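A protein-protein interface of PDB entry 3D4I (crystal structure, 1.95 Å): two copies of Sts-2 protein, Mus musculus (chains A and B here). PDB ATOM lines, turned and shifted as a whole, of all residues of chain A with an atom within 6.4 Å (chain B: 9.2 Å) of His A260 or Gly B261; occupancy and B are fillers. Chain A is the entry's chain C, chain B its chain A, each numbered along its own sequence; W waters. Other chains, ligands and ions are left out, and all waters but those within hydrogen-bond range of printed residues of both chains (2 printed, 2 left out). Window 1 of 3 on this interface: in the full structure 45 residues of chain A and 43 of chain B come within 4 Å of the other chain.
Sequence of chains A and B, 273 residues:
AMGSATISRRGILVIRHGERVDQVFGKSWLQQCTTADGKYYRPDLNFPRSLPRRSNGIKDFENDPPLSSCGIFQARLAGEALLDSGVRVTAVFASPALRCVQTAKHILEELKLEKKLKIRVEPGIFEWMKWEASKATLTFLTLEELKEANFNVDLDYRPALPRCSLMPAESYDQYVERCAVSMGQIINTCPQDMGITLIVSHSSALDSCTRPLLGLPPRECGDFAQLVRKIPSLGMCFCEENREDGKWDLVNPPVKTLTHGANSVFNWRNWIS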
ATOM      1  N   GLU A  19      28.254  -7.429  37.454  1.00  0.00           N
ATOM      2  CA  GLU A  19      29.701  -7.599  37.247  1.00  0.00           C
ATOM      3  C   GLU A  19      30.429  -6.303  37.339  1.00  0.00           C
ATOM      4  O   GLU A  19      30.041  -5.327  36.699  1.00  0.00           O
ATOM      5  CB  GLU A  19      29.952  -8.168  35.841  1.00  0.00           C
ATOM      6  CG  GLU A  19      31.388  -8.642  35.594  1.00  0.00           C
ATOM      7  CD  GLU A  19      31.589  -9.083  34.143  1.00  0.00           C
ATOM      8  OE1 GLU A  19      31.556  -8.214  33.246  1.00  0.00           O
ATOM      9  OE2 GLU A  19      31.765 -10.293  33.925  1.00  0.00           O
ATOM     10  N   VAL A  24      36.831  -8.586  35.884  1.00  0.00           N
ATOM     11  CA  VAL A  24      37.257  -9.062  34.559  1.00  0.00           C
ATOM     12  C   VAL A  24      38.694  -8.626  34.251  1.00  0.00           C
ATOM     13  O   VAL A  24      39.512  -9.423  33.772  1.00  0.00           O
ATOM     14  CB  VAL A  24      36.282  -8.545  33.454  1.00  0.00           C
ATOM     15  CG1 VAL A  24      36.741  -8.979  32.047  1.00  0.00           C
ATOM     16  CG2 VAL A  24      34.883  -9.065  33.745  1.00  0.00           C
ATOM     17  N   ASN A  46      33.842  -4.209  27.143  1.00  0.00           N
ATOM     18  CA  ASN A  46      33.303  -4.442  28.487  1.00  0.00           C
ATOM     19  C   ASN A  46      33.601  -3.330  29.492  1.00  0.00           C
ATOM     20  O   ASN A  46      33.028  -3.308  30.600  1.00  0.00           O
ATOM     21  CB  ASN A  46      33.723  -5.805  29.047  1.00  0.00           C
ATOM     22  CG  ASN A  46      32.723  -6.331  30.064  1.00  0.00           C
ATOM     23  OD1 ASN A  46      31.532  -6.053  29.964  1.00  0.00           O
ATOM     24  ND2 ASN A  46      33.203  -7.078  31.051  1.00  0.00           N
ATOM     25  N   CYS A  70      28.766  -5.750  30.705  1.00  0.00           N
ATOM     26  CA  CYS A  70      28.035  -6.967  31.012  1.00  0.00           C
ATOM     27  C   CYS A  70      27.251  -6.811  32.338  1.00  0.00           C
ATOM     28  O   CYS A  70      26.104  -7.236  32.418  1.00  0.00           O
ATOM     29  CB  CYS A  70      29.003  -8.144  31.072  1.00  0.00           C
ATOM     30  SG  CYS A  70      28.222  -9.713  31.296  1.00  0.00           S
ATOM     31  N   PHE A  73      24.199  -4.921  31.501  1.00  0.00           N
ATOM     32  CA  PHE A  73      23.264  -5.850  30.868  1.00  0.00           C
ATOM     33  C   PHE A  73      22.491  -6.704  31.876  1.00  0.00           C
ATOM     34  O   PHE A  73      21.260  -6.796  31.785  1.00  0.00           O
ATOM     35  CB  PHE A  73      23.971  -6.722  29.802  1.00  0.00           C
ATOM     36  CG  PHE A  73      23.442  -8.145  29.709  1.00  0.00           C
ATOM     37  CD1 PHE A  73      22.194  -8.416  29.139  1.00  0.00           C
ATOM     38  CD2 PHE A  73      24.222  -9.211  30.168  1.00  0.00           C
ATOM     39  CE1 PHE A  73      21.716  -9.732  29.051  1.00  0.00           C
ATOM     40  CE2 PHE A  73      23.736 -10.537  30.097  1.00  0.00           C
ATOM     41  CZ  PHE A  73      22.492 -10.785  29.560  1.00  0.00           C
ATOM     42  N   GLN A  74      23.211  -7.303  32.828  1.00  0.00           N
ATOM     43  CA  GLN A  74      22.615  -8.157  33.853  1.00  0.00           C
ATOM     44  C   GLN A  74      21.574  -7.383  34.679  1.00  0.00           C
ATOM     45  O   GLN A  74      20.462  -7.884  34.917  1.00  0.00           O
ATOM     46  CB  GLN A  74      23.721  -8.702  34.767  1.00  0.00           C
ATOM     47  CG  GLN A  74      24.689  -9.654  34.075  1.00  0.00           C
ATOM     48  CD  GLN A  74      25.964  -9.856  34.865  1.00  0.00           C
ATOM     49  OE1 GLN A  74      26.295  -9.053  35.716  1.00  0.00           O
ATOM     50  NE2 GLN A  74      26.689 -10.943  34.577  1.00  0.00           N
ATOM     51  N   LEU A  77      18.541  -6.617  32.432  1.00  0.00           N
ATOM     52  CA  LEU A  77      17.808  -7.890  32.246  1.00  0.00           C
ATOM     53  C   LEU A  77      16.945  -8.247  33.457  1.00  0.00           C
ATOM     54  O   LEU A  77      15.782  -8.650  33.311  1.00  0.00           O
ATOM     55  CB  LEU A  77      18.773  -9.045  31.929  1.00  0.00           C
ATOM     56  CG  LEU A  77      18.160 -10.355  31.391  1.00  0.00           C
ATOM     57  CD1 LEU A  77      17.492 -10.127  30.011  1.00  0.00           C
ATOM     58  CD2 LEU A  77      19.219 -11.436  31.280  1.00  0.00           C
ATOM     59  N   LEU A 258      19.697 -16.198  36.325  1.00  0.00           N
ATOM     60  CA  LEU A 258      20.371 -15.786  35.097  1.00  0.00           C
ATOM     61  C   LEU A 258      21.678 -16.549  34.998  1.00  0.00           C
ATOM     62  O   LEU A 258      22.526 -16.455  35.892  1.00  0.00           O
ATOM     63  CB  LEU A 258      20.646 -14.279  35.100  1.00  0.00           C
ATOM     64  CG  LEU A 258      21.637 -13.785  34.039  1.00  0.00           C
ATOM     65  CD1 LEU A 258      21.083 -14.029  32.639  1.00  0.00           C
ATOM     66  CD2 LEU A 258      22.053 -12.333  34.236  1.00  0.00           C
ATOM     67  N   THR A 259      21.809 -17.318  33.921  1.00  0.00           N
ATOM     68  CA  THR A 259      22.975 -18.145  33.647  1.00  0.00           C
ATOM     69  C   THR A 259      23.486 -17.755  32.248  1.00  0.00           C
ATOM     70  O   THR A 259      22.729 -17.840  31.277  1.00  0.00           O
ATOM     71  CB  THR A 259      22.564 -19.651  33.597  1.00  0.00           C
ATOM     72  OG1 THR A 259      21.854 -20.013  34.802  1.00  0.00           O
ATOM     73  CG2 THR A 259      23.792 -20.550  33.452  1.00  0.00           C
ATOM     74  N   HIS A 260      24.749 -17.349  32.131  1.00  0.00           N
ATOM     75  CA  HIS A 260      25.330 -17.088  30.800  1.00  0.00           C
ATOM     76  C   HIS A 260      26.817 -17.409  30.821  1.00  0.00           C
ATOM     77  O   HIS A 260      27.404 -17.590  31.899  1.00  0.00           O
ATOM     78  CB  HIS A 260      25.023 -15.649  30.280  1.00  0.00           C
ATOM     79  CG  HIS A 260      25.657 -14.544  31.085  1.00  0.00           C
ATOM     80  ND1 HIS A 260      27.007 -14.261  31.034  1.00  0.00           N
ATOM     81  CD2 HIS A 260      25.122 -13.658  31.962  1.00  0.00           C
ATOM     82  CE1 HIS A 260      27.267 -13.234  31.826  1.00  0.00           C
ATOM     83  NE2 HIS A 260      26.142 -12.865  32.417  1.00  0.00           N
ATOM     84  N   GLY A 261      27.426 -17.528  29.645  1.00  0.00           N
ATOM     85  CA  GLY A 261      28.819 -17.919  29.604  1.00  0.00           C
ATOM     86  C   GLY A 261      29.703 -16.701  29.530  1.00  0.00           C
ATOM     87  O   GLY A 261      29.224 -15.551  29.463  1.00  0.00           O
ATOM     88  N   ALA A 262      30.996 -16.952  29.528  1.00  0.00           N
ATOM     89  CA  ALA A 262      31.978 -15.891  29.441  1.00  0.00           C
ATOM     90  C   ALA A 262      32.212 -15.541  27.990  1.00  0.00           C
ATOM     91  O   ALA A 262      31.696 -16.217  27.078  1.00  0.00           O
ATOM     92  CB  ALA A 262      33.303 -16.322  30.109  1.00  0.00           C
ATOM     93  N   ASN A 263      32.968 -14.469  27.766  1.00  0.00           N
ATOM     94  CA  ASN A 263      33.464 -14.162  26.435  1.00  0.00           C
ATOM     95  C   ASN A 263      34.951 -13.844  26.569  1.00  0.00           C
ATOM     96  O   ASN A 263      35.338 -12.890  27.245  1.00  0.00           O
ATOM     97  CB  ASN A 263      32.710 -12.998  25.789  1.00  0.00           C
ATOM     98  CG  ASN A 263      32.618 -13.144  24.270  1.00  0.00           C
ATOM     99  OD1 ASN A 263      32.265 -14.206  23.773  1.00  0.00           O
ATOM    100  ND2 ASN A 263      32.932 -12.089  23.538  1.00  0.00           N
ATOM    101  N   GLU B  19      26.184 -15.082  21.546  1.00  0.00           N
ATOM    102  CA  GLU B  19      26.012 -16.324  22.299  1.00  0.00           C
ATOM    103  C   GLU B  19      24.676 -16.988  21.911  1.00  0.00           C
ATOM    104  O   GLU B  19      23.635 -16.334  21.868  1.00  0.00           O
ATOM    105  CB  GLU B  19      26.043 -16.023  23.798  1.00  0.00           C
ATOM    106  CG  GLU B  19      25.950 -17.290  24.662  1.00  0.00           C
ATOM    107  CD  GLU B  19      25.824 -16.934  26.130  1.00  0.00           C
ATOM    108  OE1 GLU B  19      24.718 -16.538  26.522  1.00  0.00           O
ATOM    109  OE2 GLU B  19      26.800 -17.115  26.888  1.00  0.00           O
ATOM    110  N   ARG B  20      24.734 -18.283  21.611  1.00  0.00           N
ATOM    111  CA  ARG B  20      23.539 -19.058  21.294  1.00  0.00           C
ATOM    112  C   ARG B  20      23.002 -19.790  22.538  1.00  0.00           C
ATOM    113  O   ARG B  20      23.773 -20.215  23.414  1.00  0.00           O
ATOM    114  CB  ARG B  20      23.807 -20.009  20.109  1.00  0.00           C
ATOM    115  CG  ARG B  20      25.046 -20.835  20.216  1.00  0.00           C
ATOM    116  CD  ARG B  20      25.436 -21.518  18.901  1.00  0.00           C
ATOM    117  NE  ARG B  20      24.566 -22.641  18.599  1.00  0.00           N
ATOM    118  CZ  ARG B  20      24.788 -23.515  17.617  1.00  0.00           C
ATOM    119  NH1 ARG B  20      25.888 -23.402  16.848  1.00  0.00           N
ATOM    120  NH2 ARG B  20      23.927 -24.515  17.425  1.00  0.00           N
ATOM    121  N   VAL B  21      21.673 -19.862  22.658  1.00  0.00           N
ATOM    122  CA  VAL B  21      21.061 -20.394  23.892  1.00  0.00           C
ATOM    123  C   VAL B  21      21.566 -21.783  24.196  1.00  0.00           C
ATOM    124  O   VAL B  21      21.794 -22.108  25.365  1.00  0.00           O
ATOM    125  CB  VAL B  21      19.494 -20.443  23.877  1.00  0.00           C
ATOM    126  CG1 VAL B  21      18.930 -19.068  24.143  1.00  0.00           C
ATOM    127  CG2 VAL B  21      18.968 -21.042  22.596  1.00  0.00           C
ATOM    128  N   GLN B  23      24.483 -23.041  23.708  1.00  0.00           N
ATOM    129  CA  GLN B  23      25.880 -23.086  24.198  1.00  0.00           C
ATOM    130  C   GLN B  23      25.851 -23.115  25.727  1.00  0.00           C
ATOM    131  O   GLN B  23      26.710 -23.742  26.384  1.00  0.00           O
ATOM    132  CB  GLN B  23      26.698 -21.825  23.816  1.00  0.00           C
ATOM    133  CG  GLN B  23      28.196 -22.034  24.016  1.00  0.00           C
ATOM    134  CD  GLN B  23      29.023 -20.777  23.874  1.00  0.00           C
ATOM    135  OE1 GLN B  23      28.800 -19.955  22.984  1.00  0.00           O
ATOM    136  NE2 GLN B  23      30.017 -20.637  24.742  1.00  0.00           N
ATOM    137  N   VAL B  24      24.887 -22.393  26.299  1.00  0.00           N
ATOM    138  CA  VAL B  24      24.772 -22.295  27.744  1.00  0.00           C
ATOM    139  C   VAL B  24      23.949 -23.460  28.326  1.00  0.00           C
ATOM    140  O   VAL B  24      24.333 -24.069  29.318  1.00  0.00           O
ATOM    141  CB  VAL B  24      24.155 -20.923  28.173  1.00  0.00           C
ATOM    142  CG1 VAL B  24      23.917 -20.861  29.707  1.00  0.00           C
ATOM    143  CG2 VAL B  24      25.109 -19.817  27.840  1.00  0.00           C
ATOM    144  N   PHE B  25      22.800 -23.721  27.725  1.00  0.00           N
ATOM    145  CA  PHE B  25      21.827 -24.611  28.336  1.00  0.00           C
ATOM    146  C   PHE B  25      21.932 -26.039  27.827  1.00  0.00           C
ATOM    147  O   PHE B  25      21.290 -26.954  28.370  1.00  0.00           O
ATOM    148  CB  PHE B  25      20.425 -24.026  28.206  1.00  0.00           C
ATOM    149  CG  PHE B  25      20.275 -22.728  28.975  1.00  0.00           C
ATOM    150  CD1 PHE B  25      20.197 -22.750  30.368  1.00  0.00           C
ATOM    151  CD2 PHE B  25      20.324 -21.509  28.319  1.00  0.00           C
ATOM    152  CE1 PHE B  25      20.099 -21.581  31.105  1.00  0.00           C
ATOM    153  CE2 PHE B  25      20.221 -20.304  29.047  1.00  0.00           C
ATOM    154  CZ  PHE B  25      20.121 -20.353  30.456  1.00  0.00           C
ATOM    155  N   ASP B  44      14.901 -19.414  32.556  1.00  0.00           N
ATOM    156  CA  ASP B  44      16.095 -18.683  33.029  1.00  0.00           C
ATOM    157  C   ASP B  44      16.092 -17.389  32.228  1.00  0.00           C
ATOM    158  O   ASP B  44      15.604 -17.364  31.110  1.00  0.00           O
ATOM    159  CB  ASP B  44      17.350 -19.526  32.752  1.00  0.00           C
ATOM    160  CG  ASP B  44      18.662 -18.885  33.234  1.00  0.00           C
ATOM    161  OD1 ASP B  44      19.146 -17.880  32.640  1.00  0.00           O
ATOM    162  OD2 ASP B  44      19.279 -19.468  34.156  1.00  0.00           O
ATOM    163  N   LEU B  45      16.606 -16.306  32.797  1.00  0.00           N
ATOM    164  CA  LEU B  45      16.500 -15.026  32.124  1.00  0.00           C
ATOM    165  C   LEU B  45      17.374 -14.958  30.887  1.00  0.00           C
ATOM    166  O   LEU B  45      17.202 -14.052  30.074  1.00  0.00           O
ATOM    167  CB  LEU B  45      16.818 -13.849  33.056  1.00  0.00           C
ATOM    168  CG  LEU B  45      15.991 -13.749  34.346  1.00  0.00           C
ATOM    169  CD1 LEU B  45      16.358 -12.474  35.055  1.00  0.00           C
ATOM    170  CD2 LEU B  45      14.477 -13.727  34.022  1.00  0.00           C
ATOM    171  N   ASN B  46      18.290 -15.906  30.718  1.00  0.00           N
ATOM    172  CA  ASN B  46      19.130 -15.881  29.507  1.00  0.00           C
ATOM    173  C   ASN B  46      18.461 -16.519  28.295  1.00  0.00           C
ATOM    174  O   ASN B  46      19.008 -16.443  27.195  1.00  0.00           O
ATOM    175  CB  ASN B  46      20.497 -16.516  29.768  1.00  0.00           C
ATOM    176  CG  ASN B  46      21.577 -16.045  28.799  1.00  0.00           C
ATOM    177  OD1 ASN B  46      21.620 -14.888  28.411  1.00  0.00           O
ATOM    178  ND2 ASN B  46      22.484 -16.961  28.435  1.00  0.00           N
ATOM    179  N   PHE B  47      17.306 -17.175  28.489  1.00  0.00           N
ATOM    180  CA  PHE B  47      16.417 -17.497  27.357  1.00  0.00           C
ATOM    181  C   PHE B  47      15.783 -16.202  26.904  1.00  0.00           C
ATOM    182  O   PHE B  47      15.467 -15.367  27.751  1.00  0.00           O
ATOM    183  CB  PHE B  47      15.318 -18.510  27.741  1.00  0.00           C
ATOM    184  CG  PHE B  47      15.815 -19.922  27.909  1.00  0.00           C
ATOM    185  CD1 PHE B  47      16.467 -20.316  29.070  1.00  0.00           C
ATOM    186  CD2 PHE B  47      15.620 -20.867  26.907  1.00  0.00           C
ATOM    187  CE1 PHE B  47      16.912 -21.671  29.251  1.00  0.00           C
ATOM    188  CE2 PHE B  47      16.074 -22.175  27.059  1.00  0.00           C
ATOM    189  CZ  PHE B  47      16.697 -22.588  28.235  1.00  0.00           C
ATOM    190  N   SER B  68      20.878 -16.134  22.929  1.00  0.00           N
ATOM    191  CA  SER B  68      20.491 -15.933  24.335  1.00  0.00           C
ATOM    192  C   SER B  68      20.328 -14.456  24.602  1.00  0.00           C
ATOM    193  O   SER B  68      20.705 -13.620  23.760  1.00  0.00           O
ATOM    194  CB  SER B  68      21.581 -16.483  25.243  1.00  0.00           C
ATOM    195  OG  SER B  68      22.782 -15.725  25.052  1.00  0.00           O
ATOM    196  N   SER B  69      19.783 -14.110  25.769  1.00  0.00           N
ATOM    197  CA  SER B  69      19.730 -12.705  26.189  1.00  0.00           C
ATOM    198  C   SER B  69      21.129 -12.058  26.179  1.00  0.00           C
ATOM    199  O   SER B  69      21.295 -10.905  25.771  1.00  0.00           O
ATOM    200  CB  SER B  69      19.128 -12.623  27.593  1.00  0.00           C
ATOM    201  OG  SER B  69      17.788 -13.126  27.551  1.00  0.00           O
ATOM    202  N   CYS B  70      22.130 -12.815  26.611  1.00  0.00           N
ATOM    203  CA  CYS B  70      23.516 -12.317  26.616  1.00  0.00           C
ATOM    204  C   CYS B  70      24.034 -12.126  25.169  1.00  0.00           C
ATOM    205  O   CYS B  70      24.703 -11.138  24.883  1.00  0.00           O
ATOM    206  CB  CYS B  70      24.412 -13.284  27.381  1.00  0.00           C
ATOM    207  SG  CYS B  70      26.114 -12.710  27.575  1.00  0.00           S
ATOM    208  N   GLY B  71      23.698 -13.044  24.261  1.00  0.00           N
ATOM    209  CA  GLY B  71      24.070 -12.874  22.830  1.00  0.00           C
ATOM    210  C   GLY B  71      23.488 -11.599  22.227  1.00  0.00           C
ATOM    211  O   GLY B  71      24.140 -10.903  21.435  1.00  0.00           O
ATOM    212  N   PHE B  73      22.668  -8.877  23.971  1.00  0.00           N
ATOM    213  CA  PHE B  73      23.501  -7.829  24.572  1.00  0.00           C
ATOM    214  C   PHE B  73      24.840  -7.667  23.822  1.00  0.00           C
ATOM    215  O   PHE B  73      25.231  -6.536  23.520  1.00  0.00           O
ATOM    216  CB  PHE B  73      23.706  -8.076  26.089  1.00  0.00           C
ATOM    217  CG  PHE B  73      25.107  -7.751  26.593  1.00  0.00           C
ATOM    218  CD1 PHE B  73      25.500  -6.418  26.813  1.00  0.00           C
ATOM    219  CD2 PHE B  73      26.015  -8.773  26.856  1.00  0.00           C
ATOM    220  CE1 PHE B  73      26.795  -6.125  27.280  1.00  0.00           C
ATOM    221  CE2 PHE B  73      27.331  -8.485  27.338  1.00  0.00           C
ATOM    222  CZ  PHE B  73      27.704  -7.151  27.532  1.00  0.00           C
ATOM    223  N   GLN B  74      25.534  -8.779  23.521  1.00  0.00           N
ATOM    224  CA  GLN B  74      26.819  -8.696  22.830  1.00  0.00           C
ATOM    225  C   GLN B  74      26.664  -8.041  21.452  1.00  0.00           C
ATOM    226  O   GLN B  74      27.452  -7.179  21.088  1.00  0.00           O
ATOM    227  CB  GLN B  74      27.469 -10.077  22.696  1.00  0.00           C
ATOM    228  CG  GLN B  74      27.731 -10.757  24.062  1.00  0.00           C
ATOM    229  CD  GLN B  74      27.990 -12.238  23.902  1.00  0.00           C
ATOM    230  OE1 GLN B  74      27.533 -12.856  22.944  1.00  0.00           O
ATOM    231  NE2 GLN B  74      28.740 -12.803  24.824  1.00  0.00           N
ATOM    232  N   LEU B 258      35.369  -7.745  23.060  1.00  0.00           N
ATOM    233  CA  LEU B 258      34.491  -7.745  24.208  1.00  0.00           C
ATOM    234  C   LEU B 258      34.858  -8.946  25.064  1.00  0.00           C
ATOM    235  O   LEU B 258      34.711 -10.094  24.626  1.00  0.00           O
ATOM    236  CB  LEU B 258      33.028  -7.824  23.770  1.00  0.00           C
ATOM    237  CG  LEU B 258      32.039  -8.220  24.886  1.00  0.00           C
ATOM    238  CD1 LEU B 258      31.974  -7.193  26.001  1.00  0.00           C
ATOM    239  CD2 LEU B 258      30.664  -8.493  24.245  1.00  0.00           C
ATOM    240  N   THR B 259      35.334  -8.680  26.276  1.00  0.00           N
ATOM    241  CA  THR B 259      35.731  -9.735  27.206  1.00  0.00           C
ATOM    242  C   THR B 259      34.854  -9.600  28.445  1.00  0.00           C
ATOM    243  O   THR B 259      34.812  -8.515  29.051  1.00  0.00           O
ATOM    244  CB  THR B 259      37.210  -9.537  27.662  1.00  0.00           C
ATOM    245  OG1 THR B 259      38.063  -9.309  26.521  1.00  0.00           O
ATOM    246  CG2 THR B 259      37.710 -10.749  28.461  1.00  0.00           C
ATOM    247  N   HIS B 260      34.140 -10.662  28.817  1.00  0.00           N
ATOM    248  CA  HIS B 260      33.382 -10.647  30.088  1.00  0.00           C
ATOM    249  C   HIS B 260      33.361 -12.020  30.737  1.00  0.00           C
ATOM    250  O   HIS B 260      33.726 -13.004  30.102  1.00  0.00           O
ATOM    251  CB  HIS B 260      31.932 -10.102  29.927  1.00  0.00           C
ATOM    252  CG  HIS B 260      31.050 -10.922  29.019  1.00  0.00           C
ATOM    253  ND1 HIS B 260      30.453 -12.100  29.411  1.00  0.00           N
ATOM    254  CD2 HIS B 260      30.635 -10.701  27.741  1.00  0.00           C
ATOM    255  CE1 HIS B 260      29.726 -12.584  28.418  1.00  0.00           C
ATOM    256  NE2 HIS B 260      29.825 -11.756  27.390  1.00  0.00           N
ATOM    257  N   GLY B 261      32.947 -12.089  31.998  1.00  0.00           N
ATOM    258  CA  GLY B 261      32.843 -13.373  32.716  1.00  0.00           C
ATOM    259  C   GLY B 261      31.505 -14.061  32.533  1.00  0.00           C
ATOM    260  O   GLY B 261      30.556 -13.488  31.954  1.00  0.00           O
ATOM    261  N   ALA B 262      31.431 -15.303  33.009  1.00  0.00           N
ATOM    262  CA  ALA B 262      30.201 -16.074  33.039  1.00  0.00           C
ATOM    263  C   ALA B 262      29.318 -15.612  34.201  1.00  0.00           C
ATOM    264  O   ALA B 262      29.710 -14.766  35.029  1.00  0.00           O
ATOM    265  CB  ALA B 262      30.501 -17.628  33.132  1.00  0.00           C
ATOM    266  N   ASN B 263      28.103 -16.130  34.221  1.00  0.00           N
ATOM    267  CA  ASN B 263      27.245 -15.990  35.377  1.00  0.00           C
ATOM    268  C   ASN B 263      26.673 -17.359  35.687  1.00  0.00           C
ATOM    269  O   ASN B 263      26.009 -17.959  34.842  1.00  0.00           O
ATOM    270  CB  ASN B 263      26.150 -14.972  35.118  1.00  0.00           C
ATOM    271  CG  ASN B 263      25.290 -14.695  36.358  1.00  0.00           C
ATOM    272  OD1 ASN B 263      25.060 -13.562  36.709  1.00  0.00           O
ATOM    273  ND2 ASN B 263      24.808 -15.738  36.995  1.00  0.00           N
ATOM    274  N   SER B 264      26.931 -17.857  36.894  1.00  0.00           N
ATOM    275  CA  SER B 264      26.487 -19.202  37.261  1.00  0.00           C
ATOM    276  C   SER B 264      25.002 -19.239  37.560  1.00  0.00           C
ATOM    277  O   SER B 264      24.427 -18.232  37.997  1.00  0.00           O
ATOM    278  CB  SER B 264      27.206 -19.673  38.515  1.00  0.00           C
ATOM    279  OG  SER B 264      26.571 -19.053  39.640  1.00  0.00           O
ATOM    280  N   VAL B 265      24.395 -20.416  37.358  1.00  0.00           N
ATOM    281  CA  VAL B 265      23.031 -20.682  37.820  1.00  0.00           C
ATOM    282  C   VAL B 265      23.023 -20.554  39.356  1.00  0.00           C
ATOM    283  O   VAL B 265      24.036 -20.849  39.990  1.00  0.00           O
ATOM    284  CB  VAL B 265      22.523 -22.090  37.334  1.00  0.00           C
ATOM    285  CG1 VAL B 265      23.292 -23.245  38.000  1.00  0.00           C
ATOM    286  CG2 VAL B 265      21.022 -22.247  37.535  1.00  0.00           C
ATOM    287  N   PHE B 266      21.912 -20.088  39.936  1.00  0.00           N
ATOM    288  CA  PHE B 266      21.834 -19.820  41.386  1.00  0.00           C
ATOM    289  C   PHE B 266      20.427 -19.879  41.990  1.00  0.00           C
ATOM    290  O   PHE B 266      19.499 -19.209  41.529  1.00  0.00           O
ATOM    291  CB  PHE B 266      22.423 -18.438  41.683  1.00  0.00           C
ATOM    292  CG  PHE B 266      22.294 -18.000  43.114  1.00  0.00           C
ATOM    293  CD1 PHE B 266      23.099 -18.557  44.101  1.00  0.00           C
ATOM    294  CD2 PHE B 266      21.396 -17.001  43.471  1.00  0.00           C
ATOM    295  CE1 PHE B 266      22.998 -18.131  45.428  1.00  0.00           C
ATOM    296  CE2 PHE B 266      21.291 -16.571  44.788  1.00  0.00           C
ATOM    297  CZ  PHE B 266      22.090 -17.138  45.767  1.00  0.00           C
HETATM  298  O   HOH W   1      36.449 -13.881  29.873  1.00  0.00           O
HETATM  299  O   HOH W   2      27.485 -20.291  33.662  1.00  0.00           O
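The backbone NH (N) of Gly A261 is in hydrogen-bond range of the side-chain carboxylate (OE2) of Glu B19 (2.9 Å). The side-chain hydroxyl (OG1) of Thr A259 is in hydrogen-bond range of the side-chain carboxylate (OD2) of Asp B44 (2.7 Å). The side-chain amide nitrogen (ND2) of Asn B46 sits at hydrogen-bond distance from the backbone carbonyl oxygen (O) of Thr A259 (3.0 Å). The side-chain amide nitrogen of Asn A263 sits at hydrogen-bond distance from the backbone carbonyl oxygen of Leu B258 (2.9 Å). The side-chain amide nitrogen of Asn A46 lies close to the backbone carbonyl oxygen of Thr B259 (2.9 Å). The side-chain sulfur (SG) of Cys A70 sits at hydrogen-bond distance from a ring nitrogen (ND1) of His B260, at 3.8 Å. The backbone NH of Asn A263 is in hydrogen-bond range of the backbone carbonyl oxygen of His B260. The backbone NH of Gly B261 lies within hydrogen-bond range of the side-chain carboxylate of Glu A19 (2.9 Å). ND2 of Asn B263 sits at hydrogen-bond distance from O of Leu A258, at 2.6 Å. O of His A260 sits at hydrogen-bond distance from N of Asn B263, 2.8 Å away. O of Leu A258 sits close to O of Ser B264, 3.3 Å away. The backbone carbonyl oxygen (O) of Gly A261 lies close to the backbone carbonyl oxygen (O) of Gly B261, 3.5 Å away.
Thr B259 touches Val A24. Val A24 touches Gly B261 (CG2 to N, 3.99 Å). Cys A70 touches Phe B73 (CA to CZ, 3.5 Å). Phe A73 touches Phe B73. Asp B44 touches Leu A258. CB of Cys B70 touches CB of His A260, at 3.8 Å. Gly A261 touches His B260. Ala A262 touches Ala B262. Thr B259 touches Asn A263.
Hydrophobic or aromatic side chains of chain B that line the printed part of chain A: Val B24, Phe B25, Leu B45, Phe B73, Leu B258, His B260, Ala B262 and Val B265. Of the 13 printed residues of chain A, 13 touch a printed residue of chain B. Among the printed residues, no Asp or Glu carboxylate lies within 4 Å of a Lys or Arg side-chain nitrogen of the other chain.
OD1 of Asn B46 sits at hydrogen-bond distance from N of Cys B70 (2.8 Å). The side-chain amide nitrogen (NE2) of Gln A74 is in hydrogen-bond range of a ring nitrogen (NE2) of His A260, at 2.9 Å.
Of chain B, only Val B24 (3.6 Å), Phe B25 (3.7 Å), Asp B44 (2.7 Å), Asn B46 (3.0 Å), Asn B263 (3.3 Å) and Val B265 (3.3 Å) come within 4 Å of Thr A259. Of the printed residues of chain A, Leu B45 touches Leu A77. Ser B68 touches none of the printed residues of chain A. Of the printed residues of chain A, Leu B258 touches Asn A46 (3.7 Å) and Asn A263 (2.9 Å). Of the printed residues of chain A, Ser B264 touches Leu A258 (3.3 Å). The nearest printed residue of chain B that does not touch Gln A74 is Ala B262 (4.9 Å).
Water W1 lies within hydrogen-bond range of the backbone carbonyl oxygen (O) of His B260 (2.9 Å) and the backbone carbonyl oxygen (O) of Asn A263 (3.0 Å). Water W2 bridges O of Asn B263 (3.0 Å) and O of His A260 (3.2 Å).
Cys A70 touches His B260, and with the chains exchanged His A260 touches Cys B70. Thr A259 touches Asn B263, and with the chains exchanged Asn A263 touches Thr B259. His A260 touches Gly B261, and with the chains exchanged Gly A261 touches His B260. Ala A262 touches its own counterpart, Ala B262.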
